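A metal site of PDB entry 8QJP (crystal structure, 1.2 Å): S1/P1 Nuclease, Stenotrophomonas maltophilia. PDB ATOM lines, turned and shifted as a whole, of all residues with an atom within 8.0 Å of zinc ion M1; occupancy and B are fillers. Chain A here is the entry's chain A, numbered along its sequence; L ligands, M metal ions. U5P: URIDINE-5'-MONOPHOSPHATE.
ND1 of His 125 sits close to O2 of the ligand, at 3.5 Å.
The side-chain carboxylate (OD1) of Asp 153 lies close to the backbone NH (N) of Trp 1 (3.0 Å). N of Gly 2 sits at hydrogen-bond distance from O of Asp 153 (3.1 Å). A ring nitrogen (ND1) of His 125 sits at hydrogen-bond distance from the backbone carbonyl oxygen of His 62 (2.7 Å). ND1 of His 149 lies within hydrogen-bond range of ND2 of Asn 135 (3.4 Å). A ring nitrogen (ND1) of His 149 is in hydrogen-bond range of the backbone carbonyl oxygen (O) of Met 124 (3.3 Å). A ring nitrogen (ND1) of His 149 sits at hydrogen-bond distance from the backbone carbonyl oxygen (O) of Gly 133 (2.8 Å). The backbone NH (N) of His 149 sits at hydrogen-bond distance from the side-chain amide oxygen (OD1) of Asn 147.
Within 4 Å of zinc ion M1: His 125, His 149 and Asp 153.
Zinc ion M1 is bound by OD2 of Asp 153, NE2 of His 125 and NE2 of His 149. Zinc ion M1 has three donor atoms within binding distance.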
ATOM      1  N   TRP A   1      -2.527   5.360 -20.168  1.00  0.00           N
ATOM      2  CA  TRP A   1      -1.913   5.564 -18.852  1.00  0.00           C
ATOM      3  C   TRP A   1      -2.919   6.229 -17.946  1.00  0.00           C
ATOM      4  O   TRP A   1      -3.871   6.882 -18.430  1.00  0.00           O
ATOM      5  CB  TRP A   1      -0.655   6.468 -18.930  1.00  0.00           C
ATOM      6  CG  TRP A   1       0.390   5.995 -19.886  1.00  0.00           C
ATOM      7  CD1 TRP A   1       0.570   6.394 -21.174  1.00  0.00           C
ATOM      8  CD2 TRP A   1       1.399   5.010 -19.632  1.00  0.00           C
ATOM      9  NE1 TRP A   1       1.648   5.769 -21.734  1.00  0.00           N
ATOM     10  CE2 TRP A   1       2.179   4.895 -20.814  1.00  0.00           C
ATOM     11  CE3 TRP A   1       1.750   4.243 -18.516  1.00  0.00           C
ATOM     12  CZ2 TRP A   1       3.259   4.040 -20.916  1.00  0.00           C
ATOM     13  CZ3 TRP A   1       2.828   3.419 -18.604  1.00  0.00           C
ATOM     14  CH2 TRP A   1       3.547   3.298 -19.797  1.00  0.00           C
ATOM     15  N   GLY A   2      -2.657   6.147 -16.646  1.00  0.00           N
ATOM     16  CA  GLY A   2      -3.281   7.046 -15.665  1.00  0.00           C
ATOM     17  C   GLY A   2      -2.664   8.422 -15.722  1.00  0.00           C
ATOM     18  O   GLY A   2      -1.781   8.693 -16.568  1.00  0.00           O
ATOM     19  N   HIS A   6       0.637  10.137 -18.013  1.00  0.00           N
ATOM     20  CA  HIS A   6       0.401  11.188 -19.022  1.00  0.00           C
ATOM     21  C   HIS A   6       1.233  12.448 -18.735  1.00  0.00           C
ATOM     22  O   HIS A   6       1.848  13.002 -19.646  1.00  0.00           O
ATOM     23  CB  HIS A   6      -1.083  11.531 -19.151  1.00  0.00           C
ATOM     24  CG  HIS A   6      -1.784  10.470 -19.925  1.00  0.00           C
ATOM     25  ND1 HIS A   6      -1.570  10.319 -21.281  1.00  0.00           N
ATOM     26  CD2 HIS A   6      -2.629   9.485 -19.560  1.00  0.00           C
ATOM     27  CE1 HIS A   6      -2.280   9.267 -21.698  1.00  0.00           C
ATOM     28  NE2 HIS A   6      -2.917   8.706 -20.655  1.00  0.00           N
ATOM     29  N   ASP A  45      -8.765  12.222 -20.639  1.00  0.00           N
ATOM     30  CA  ASP A  45      -9.418  11.173 -19.787  1.00  0.00           C
ATOM     31  C   ASP A  45     -10.491  11.750 -18.866  1.00  0.00           C
ATOM     32  O   ASP A  45     -11.251  10.942 -18.273  1.00  0.00           O
ATOM     33  CB  ASP A  45      -8.376  10.415 -18.979  1.00  0.00           C
ATOM     34  CG  ASP A  45      -7.586   9.364 -19.722  1.00  0.00           C
ATOM     35  OD1 ASP A  45      -7.923   9.045 -20.867  1.00  0.00           O
ATOM     36  OD2 ASP A  45      -6.568   8.857 -19.172  1.00  0.00           O
ATOM     37  N   HIS A  62      -8.648   6.544 -27.596  1.00  0.00           N
ATOM     38  CA  HIS A  62      -7.528   6.266 -26.656  1.00  0.00           C
ATOM     39  C   HIS A  62      -6.828   4.951 -26.961  1.00  0.00           C
ATOM     40  O   HIS A  62      -5.801   4.684 -26.294  1.00  0.00           O
ATOM     41  CB  HIS A  62      -8.005   6.316 -25.220  1.00  0.00           C
ATOM     42  CG  HIS A  62      -8.482   7.654 -24.799  1.00  0.00           C
ATOM     43  ND1 HIS A  62      -7.950   8.329 -23.711  1.00  0.00           N
ATOM     44  CD2 HIS A  62      -9.498   8.410 -25.283  1.00  0.00           C
ATOM     45  CE1 HIS A  62      -8.579   9.498 -23.607  1.00  0.00           C
ATOM     46  NE2 HIS A  62      -9.538   9.561 -24.563  1.00  0.00           N
ATOM     47  N   TYR A  63      -7.350   4.126 -27.853  1.00  0.00           N
ATOM     48  CA  TYR A  63      -6.756   2.785 -28.039  1.00  0.00           C
ATOM     49  C   TYR A  63      -7.000   2.250 -29.443  1.00  0.00           C
ATOM     50  O   TYR A  63      -7.715   2.853 -30.237  1.00  0.00           O
ATOM     51  CB  TYR A  63      -7.272   1.837 -26.977  1.00  0.00           C
ATOM     52  CG  TYR A  63      -8.756   1.722 -26.995  1.00  0.00           C
ATOM     53  CD1 TYR A  63      -9.552   2.619 -26.306  1.00  0.00           C
ATOM     54  CD2 TYR A  63      -9.378   0.694 -27.694  1.00  0.00           C
ATOM     55  CE1 TYR A  63     -10.931   2.502 -26.369  1.00  0.00           C
ATOM     56  CE2 TYR A  63     -10.745   0.550 -27.740  1.00  0.00           C
ATOM     57  CZ  TYR A  63     -11.537   1.459 -27.069  1.00  0.00           C
ATOM     58  OH  TYR A  63     -12.894   1.274 -27.150  1.00  0.00           O
ATOM     59  N   HIS A 115      -1.951  13.828 -25.035  1.00  0.00           N
ATOM     60  CA  HIS A 115      -2.523  12.642 -24.364  1.00  0.00           C
ATOM     61  C   HIS A 115      -2.276  11.396 -25.224  1.00  0.00           C
ATOM     62  O   HIS A 115      -1.899  10.337 -24.714  1.00  0.00           O
ATOM     63  CB  HIS A 115      -4.013  12.852 -24.131  1.00  0.00           C
ATOM     64  CG  HIS A 115      -4.613  11.784 -23.302  1.00  0.00           C
ATOM     65  ND1 HIS A 115      -4.635  11.864 -21.932  1.00  0.00           N
ATOM     66  CD2 HIS A 115      -5.180  10.595 -23.611  1.00  0.00           C
ATOM     67  CE1 HIS A 115      -5.211  10.773 -21.444  1.00  0.00           C
ATOM     68  NE2 HIS A 115      -5.560   9.956 -22.464  1.00  0.00           N
ATOM     69  N   ASP A 119      -0.873   7.582 -24.771  1.00  0.00           N
ATOM     70  CA  ASP A 119      -1.684   6.346 -24.814  1.00  0.00           C
ATOM     71  C   ASP A 119      -1.184   5.386 -25.894  1.00  0.00           C
ATOM     72  O   ASP A 119      -1.231   4.164 -25.689  1.00  0.00           O
ATOM     73  CB  ASP A 119      -3.161   6.637 -25.030  1.00  0.00           C
ATOM     74  CG  ASP A 119      -3.939   6.861 -23.760  1.00  0.00           C
ATOM     75  OD1 ASP A 119      -3.342   6.609 -22.650  1.00  0.00           O
ATOM     76  OD2 ASP A 119      -5.114   7.352 -23.836  1.00  0.00           O
ATOM     77  N   GLN A 122       1.301   3.048 -24.548  1.00  0.00           N
ATOM     78  CA  GLN A 122       0.890   2.141 -23.465  1.00  0.00           C
ATOM     79  C   GLN A 122       0.526   0.798 -24.073  1.00  0.00           C
ATOM     80  O   GLN A 122      -0.441   0.725 -24.832  1.00  0.00           O
ATOM     81  CB  GLN A 122      -0.258   2.794 -22.726  1.00  0.00           C
ATOM     82  CG  GLN A 122      -1.012   1.832 -21.837  1.00  0.00           C
ATOM     83  CD  GLN A 122      -0.125   1.035 -20.919  1.00  0.00           C
ATOM     84  OE1 GLN A 122      -0.079  -0.191 -20.984  1.00  0.00           O
ATOM     85  NE2 GLN A 122       0.617   1.752 -20.080  1.00  0.00           N
ATOM     86  N   MET A 124      -1.084  -1.801 -23.256  1.00  0.00           N
ATOM     87  CA  MET A 124      -2.472  -2.280 -23.037  1.00  0.00           C
ATOM     88  C   MET A 124      -3.512  -1.364 -23.703  1.00  0.00           C
ATOM     89  O   MET A 124      -4.693  -1.716 -23.679  1.00  0.00           O
ATOM     90  CB  MET A 124      -2.776  -2.423 -21.548  1.00  0.00           C
ATOM     91  CG  MET A 124      -1.945  -3.473 -20.894  1.00  0.00           C
ATOM     92  SD  MET A 124      -2.397  -5.141 -21.453  1.00  0.00           S
ATOM     93  CE  MET A 124      -0.790  -5.916 -21.388  1.00  0.00           C
ATOM     94  N   HIS A 125      -3.078  -0.266 -24.318  1.00  0.00           N
ATOM     95  CA  HIS A 125      -3.920   0.551 -25.225  1.00  0.00           C
ATOM     96  C   HIS A 125      -3.782   0.086 -26.684  1.00  0.00           C
ATOM     97  O   HIS A 125      -4.380   0.731 -27.567  1.00  0.00           O
ATOM     98  CB  HIS A 125      -3.612   2.036 -25.045  1.00  0.00           C
ATOM     99  CG  HIS A 125      -4.264   2.620 -23.821  1.00  0.00           C
ATOM    100  ND1 HIS A 125      -5.137   3.692 -23.864  1.00  0.00           N
ATOM    101  CD2 HIS A 125      -4.190   2.265 -22.491  1.00  0.00           C
ATOM    102  CE1 HIS A 125      -5.599   3.960 -22.652  1.00  0.00           C
ATOM    103  NE2 HIS A 125      -5.037   3.097 -21.763  1.00  0.00           N
ATOM    104  N   LYS A 132     -10.742  -6.265 -23.831  1.00  0.00           N
ATOM    105  CA  LYS A 132     -10.726  -4.798 -23.686  1.00  0.00           C
ATOM    106  C   LYS A 132      -9.339  -4.352 -23.192  1.00  0.00           C
ATOM    107  O   LYS A 132      -9.236  -3.607 -22.222  1.00  0.00           O
ATOM    108  CB  LYS A 132     -11.872  -4.320 -22.786  1.00  0.00           C
ATOM    109  CG  LYS A 132     -13.261  -4.616 -23.345  1.00  0.00           C
ATOM    110  CD  LYS A 132     -14.417  -4.242 -22.428  1.00  0.00           C
ATOM    111  CE  LYS A 132     -15.666  -5.074 -22.670  1.00  0.00           C
ATOM    112  NZ  LYS A 132     -15.986  -5.239 -24.107  1.00  0.00           N
ATOM    113  N   GLY A 133      -8.312  -4.742 -23.912  1.00  0.00           N
ATOM    114  CA  GLY A 133      -6.949  -4.260 -23.633  1.00  0.00           C
ATOM    115  C   GLY A 133      -6.472  -4.722 -22.268  1.00  0.00           C
ATOM    116  O   GLY A 133      -5.836  -3.933 -21.539  1.00  0.00           O
ATOM    117  N   ASN A 135      -8.352  -5.140 -19.637  1.00  0.00           N
ATOM    118  CA  ASN A 135      -9.245  -4.675 -18.563  1.00  0.00           C
ATOM    119  C   ASN A 135      -9.981  -5.883 -17.968  1.00  0.00           C
ATOM    120  O   ASN A 135     -10.191  -5.917 -16.745  1.00  0.00           O
ATOM    121  CB  ASN A 135     -10.235  -3.638 -19.061  1.00  0.00           C
ATOM    122  CG  ASN A 135      -9.680  -2.224 -19.116  1.00  0.00           C
ATOM    123  OD1 ASN A 135      -9.433  -1.613 -18.069  1.00  0.00           O
ATOM    124  ND2 ASN A 135      -9.481  -1.674 -20.305  1.00  0.00           N
ATOM    125  N   ASN A 147      -6.483  -5.253 -12.392  1.00  0.00           N
ATOM    126  CA  ASN A 147      -6.573  -5.913 -13.700  1.00  0.00           C
ATOM    127  C   ASN A 147      -5.327  -5.546 -14.499  1.00  0.00           C
ATOM    128  O   ASN A 147      -4.603  -4.603 -14.103  1.00  0.00           O
ATOM    129  CB  ASN A 147      -7.888  -5.567 -14.412  1.00  0.00           C
ATOM    130  CG  ASN A 147      -8.020  -4.108 -14.737  1.00  0.00           C
ATOM    131  OD1 ASN A 147      -7.259  -3.583 -15.522  1.00  0.00           O
ATOM    132  ND2 ASN A 147      -9.059  -3.483 -14.229  1.00  0.00           N
ATOM    133  N   HIS A 149      -4.809  -4.211 -17.372  1.00  0.00           N
ATOM    134  CA  HIS A 149      -4.843  -2.870 -17.967  1.00  0.00           C
ATOM    135  C   HIS A 149      -4.380  -1.815 -16.947  1.00  0.00           C
ATOM    136  O   HIS A 149      -3.475  -1.050 -17.218  1.00  0.00           O
ATOM    137  CB  HIS A 149      -6.216  -2.551 -18.551  1.00  0.00           C
ATOM    138  CG  HIS A 149      -6.207  -1.288 -19.336  1.00  0.00           C
ATOM    139  ND1 HIS A 149      -6.137  -1.277 -20.702  1.00  0.00           N
ATOM    140  CD2 HIS A 149      -6.244   0.008 -18.934  1.00  0.00           C
ATOM    141  CE1 HIS A 149      -6.108  -0.034 -21.114  1.00  0.00           C
ATOM    142  NE2 HIS A 149      -6.180   0.805 -20.064  1.00  0.00           N
ATOM    143  N   SER A 150      -5.025  -1.809 -15.792  1.00  0.00           N
ATOM    144  CA  SER A 150      -4.712  -0.849 -14.719  1.00  0.00           C
ATOM    145  C   SER A 150      -3.286  -1.085 -14.205  1.00  0.00           C
ATOM    146  O   SER A 150      -2.598  -0.091 -13.874  1.00  0.00           O
ATOM    147  CB  SER A 150      -5.712  -0.933 -13.632  1.00  0.00           C
ATOM    148  OG  SER A 150      -6.972  -0.469 -14.070  1.00  0.00           O
ATOM    149  N   TRP A 152      -0.664  -1.830 -15.879  1.00  0.00           N
ATOM    150  CA  TRP A 152       0.206  -1.165 -16.849  1.00  0.00           C
ATOM    151  C   TRP A 152      -0.065   0.345 -16.875  1.00  0.00           C
ATOM    152  O   TRP A 152       0.895   1.090 -17.044  1.00  0.00           O
ATOM    153  CB  TRP A 152       0.063  -1.830 -18.231  1.00  0.00           C
ATOM    154  CG  TRP A 152       0.902  -3.064 -18.312  1.00  0.00           C
ATOM    155  CD1 TRP A 152       0.635  -4.299 -17.851  1.00  0.00           C
ATOM    156  CD2 TRP A 152       2.252  -3.089 -18.812  1.00  0.00           C
ATOM    157  NE1 TRP A 152       1.710  -5.126 -18.033  1.00  0.00           N
ATOM    158  CE2 TRP A 152       2.717  -4.414 -18.622  1.00  0.00           C
ATOM    159  CE3 TRP A 152       3.113  -2.147 -19.371  1.00  0.00           C
ATOM    160  CZ2 TRP A 152       3.992  -4.802 -19.012  1.00  0.00           C
ATOM    161  CZ3 TRP A 152       4.360  -2.546 -19.747  1.00  0.00           C
ATOM    162  CH2 TRP A 152       4.828  -3.834 -19.549  1.00  0.00           C
ATOM    163  N   ASP A 153      -1.297   0.795 -16.768  1.00  0.00           N
ATOM    164  CA  ASP A 153      -1.593   2.244 -16.780  1.00  0.00           C
ATOM    165  C   ASP A 153      -0.991   2.941 -15.581  1.00  0.00           C
ATOM    166  O   ASP A 153      -0.558   4.095 -15.724  1.00  0.00           O
ATOM    167  CB  ASP A 153      -3.107   2.528 -16.807  1.00  0.00           C
ATOM    168  CG  ASP A 153      -3.747   2.653 -18.189  1.00  0.00           C
ATOM    169  OD1 ASP A 153      -3.039   2.525 -19.188  1.00  0.00           O
ATOM    170  OD2 ASP A 153      -4.957   2.858 -18.227  1.00  0.00           O
ATOM    171  N   SER A 154      -1.046   2.311 -14.415  1.00  0.00           N
ATOM    172  CA  SER A 154      -0.623   3.000 -13.166  1.00  0.00           C
ATOM    173  C   SER A 154      -0.098   2.081 -12.070  1.00  0.00           C
ATOM    174  O   SER A 154       0.674   2.573 -11.260  1.00  0.00           O
ATOM    175  CB  SER A 154      -1.716   3.836 -12.632  1.00  0.00           C
ATOM    176  OG  SER A 154      -2.843   3.084 -12.328  1.00  0.00           O
HETATM  177  N1  U5P L   1     -10.166   1.630 -22.888  1.00  0.00           N
HETATM  178  C2  U5P L   1      -8.998   1.093 -23.388  1.00  0.00           C
HETATM  179  N3  U5P L   1      -9.152  -0.078 -24.100  1.00  0.00           N
HETATM  180  C4  U5P L   1     -10.330  -0.738 -24.366  1.00  0.00           C
HETATM  181  C5  U5P L   1     -11.497  -0.154 -23.759  1.00  0.00           C
HETATM  182  C6  U5P L   1     -11.380   0.997 -23.051  1.00  0.00           C
HETATM  183  O2  U5P L   1      -7.898   1.638 -23.289  1.00  0.00           O
HETATM  184  O4  U5P L   1     -10.310  -1.738 -25.076  1.00  0.00           O
HETATM  185  C1' U5P L   1     -10.086   2.943 -22.140  1.00  0.00           C
HETATM  186  C2' U5P L   1      -9.980   4.136 -23.071  1.00  0.00           C
HETATM  187  O2' U5P L   1      -9.128   5.103 -22.452  1.00  0.00           O
HETATM  188  C3' U5P L   1     -11.426   4.618 -23.149  1.00  0.00           C
HETATM  189  C4' U5P L   1     -11.918   4.360 -21.735  1.00  0.00           C
HETATM  190  O3' U5P L   1     -11.581   5.996 -23.446  1.00  0.00           O
HETATM  191  O4' U5P L   1     -11.249   3.139 -21.359  1.00  0.00           O
HETATM  192  C5' U5P L   1     -13.406   4.238 -21.552  1.00  0.00           C
HETATM  193  O5' U5P L   1     -13.929   3.235 -22.447  1.00  0.00           O
HETATM  194  P   U5P L   1     -15.403   2.729 -22.254  1.00  0.00           P
HETATM  195  O1P U5P L   1     -15.773   2.041 -23.540  1.00  0.00           O
HETATM  196  O2P U5P L   1     -16.289   3.952 -22.015  1.00  0.00           O
HETATM  197  O3P U5P L   1     -15.456   1.919 -20.967  1.00  0.00           O
HETATM  198 ZN    ZN M   1      -5.814   2.765 -19.956  1.00  0.00          ZN
HETATM  199 ZN    ZN M   2      -3.875   6.903 -20.673  1.00  0.00          ZN
HETATM  200 ZN    ZN M   3      -6.427   8.086 -22.398  1.00  0.00          ZN
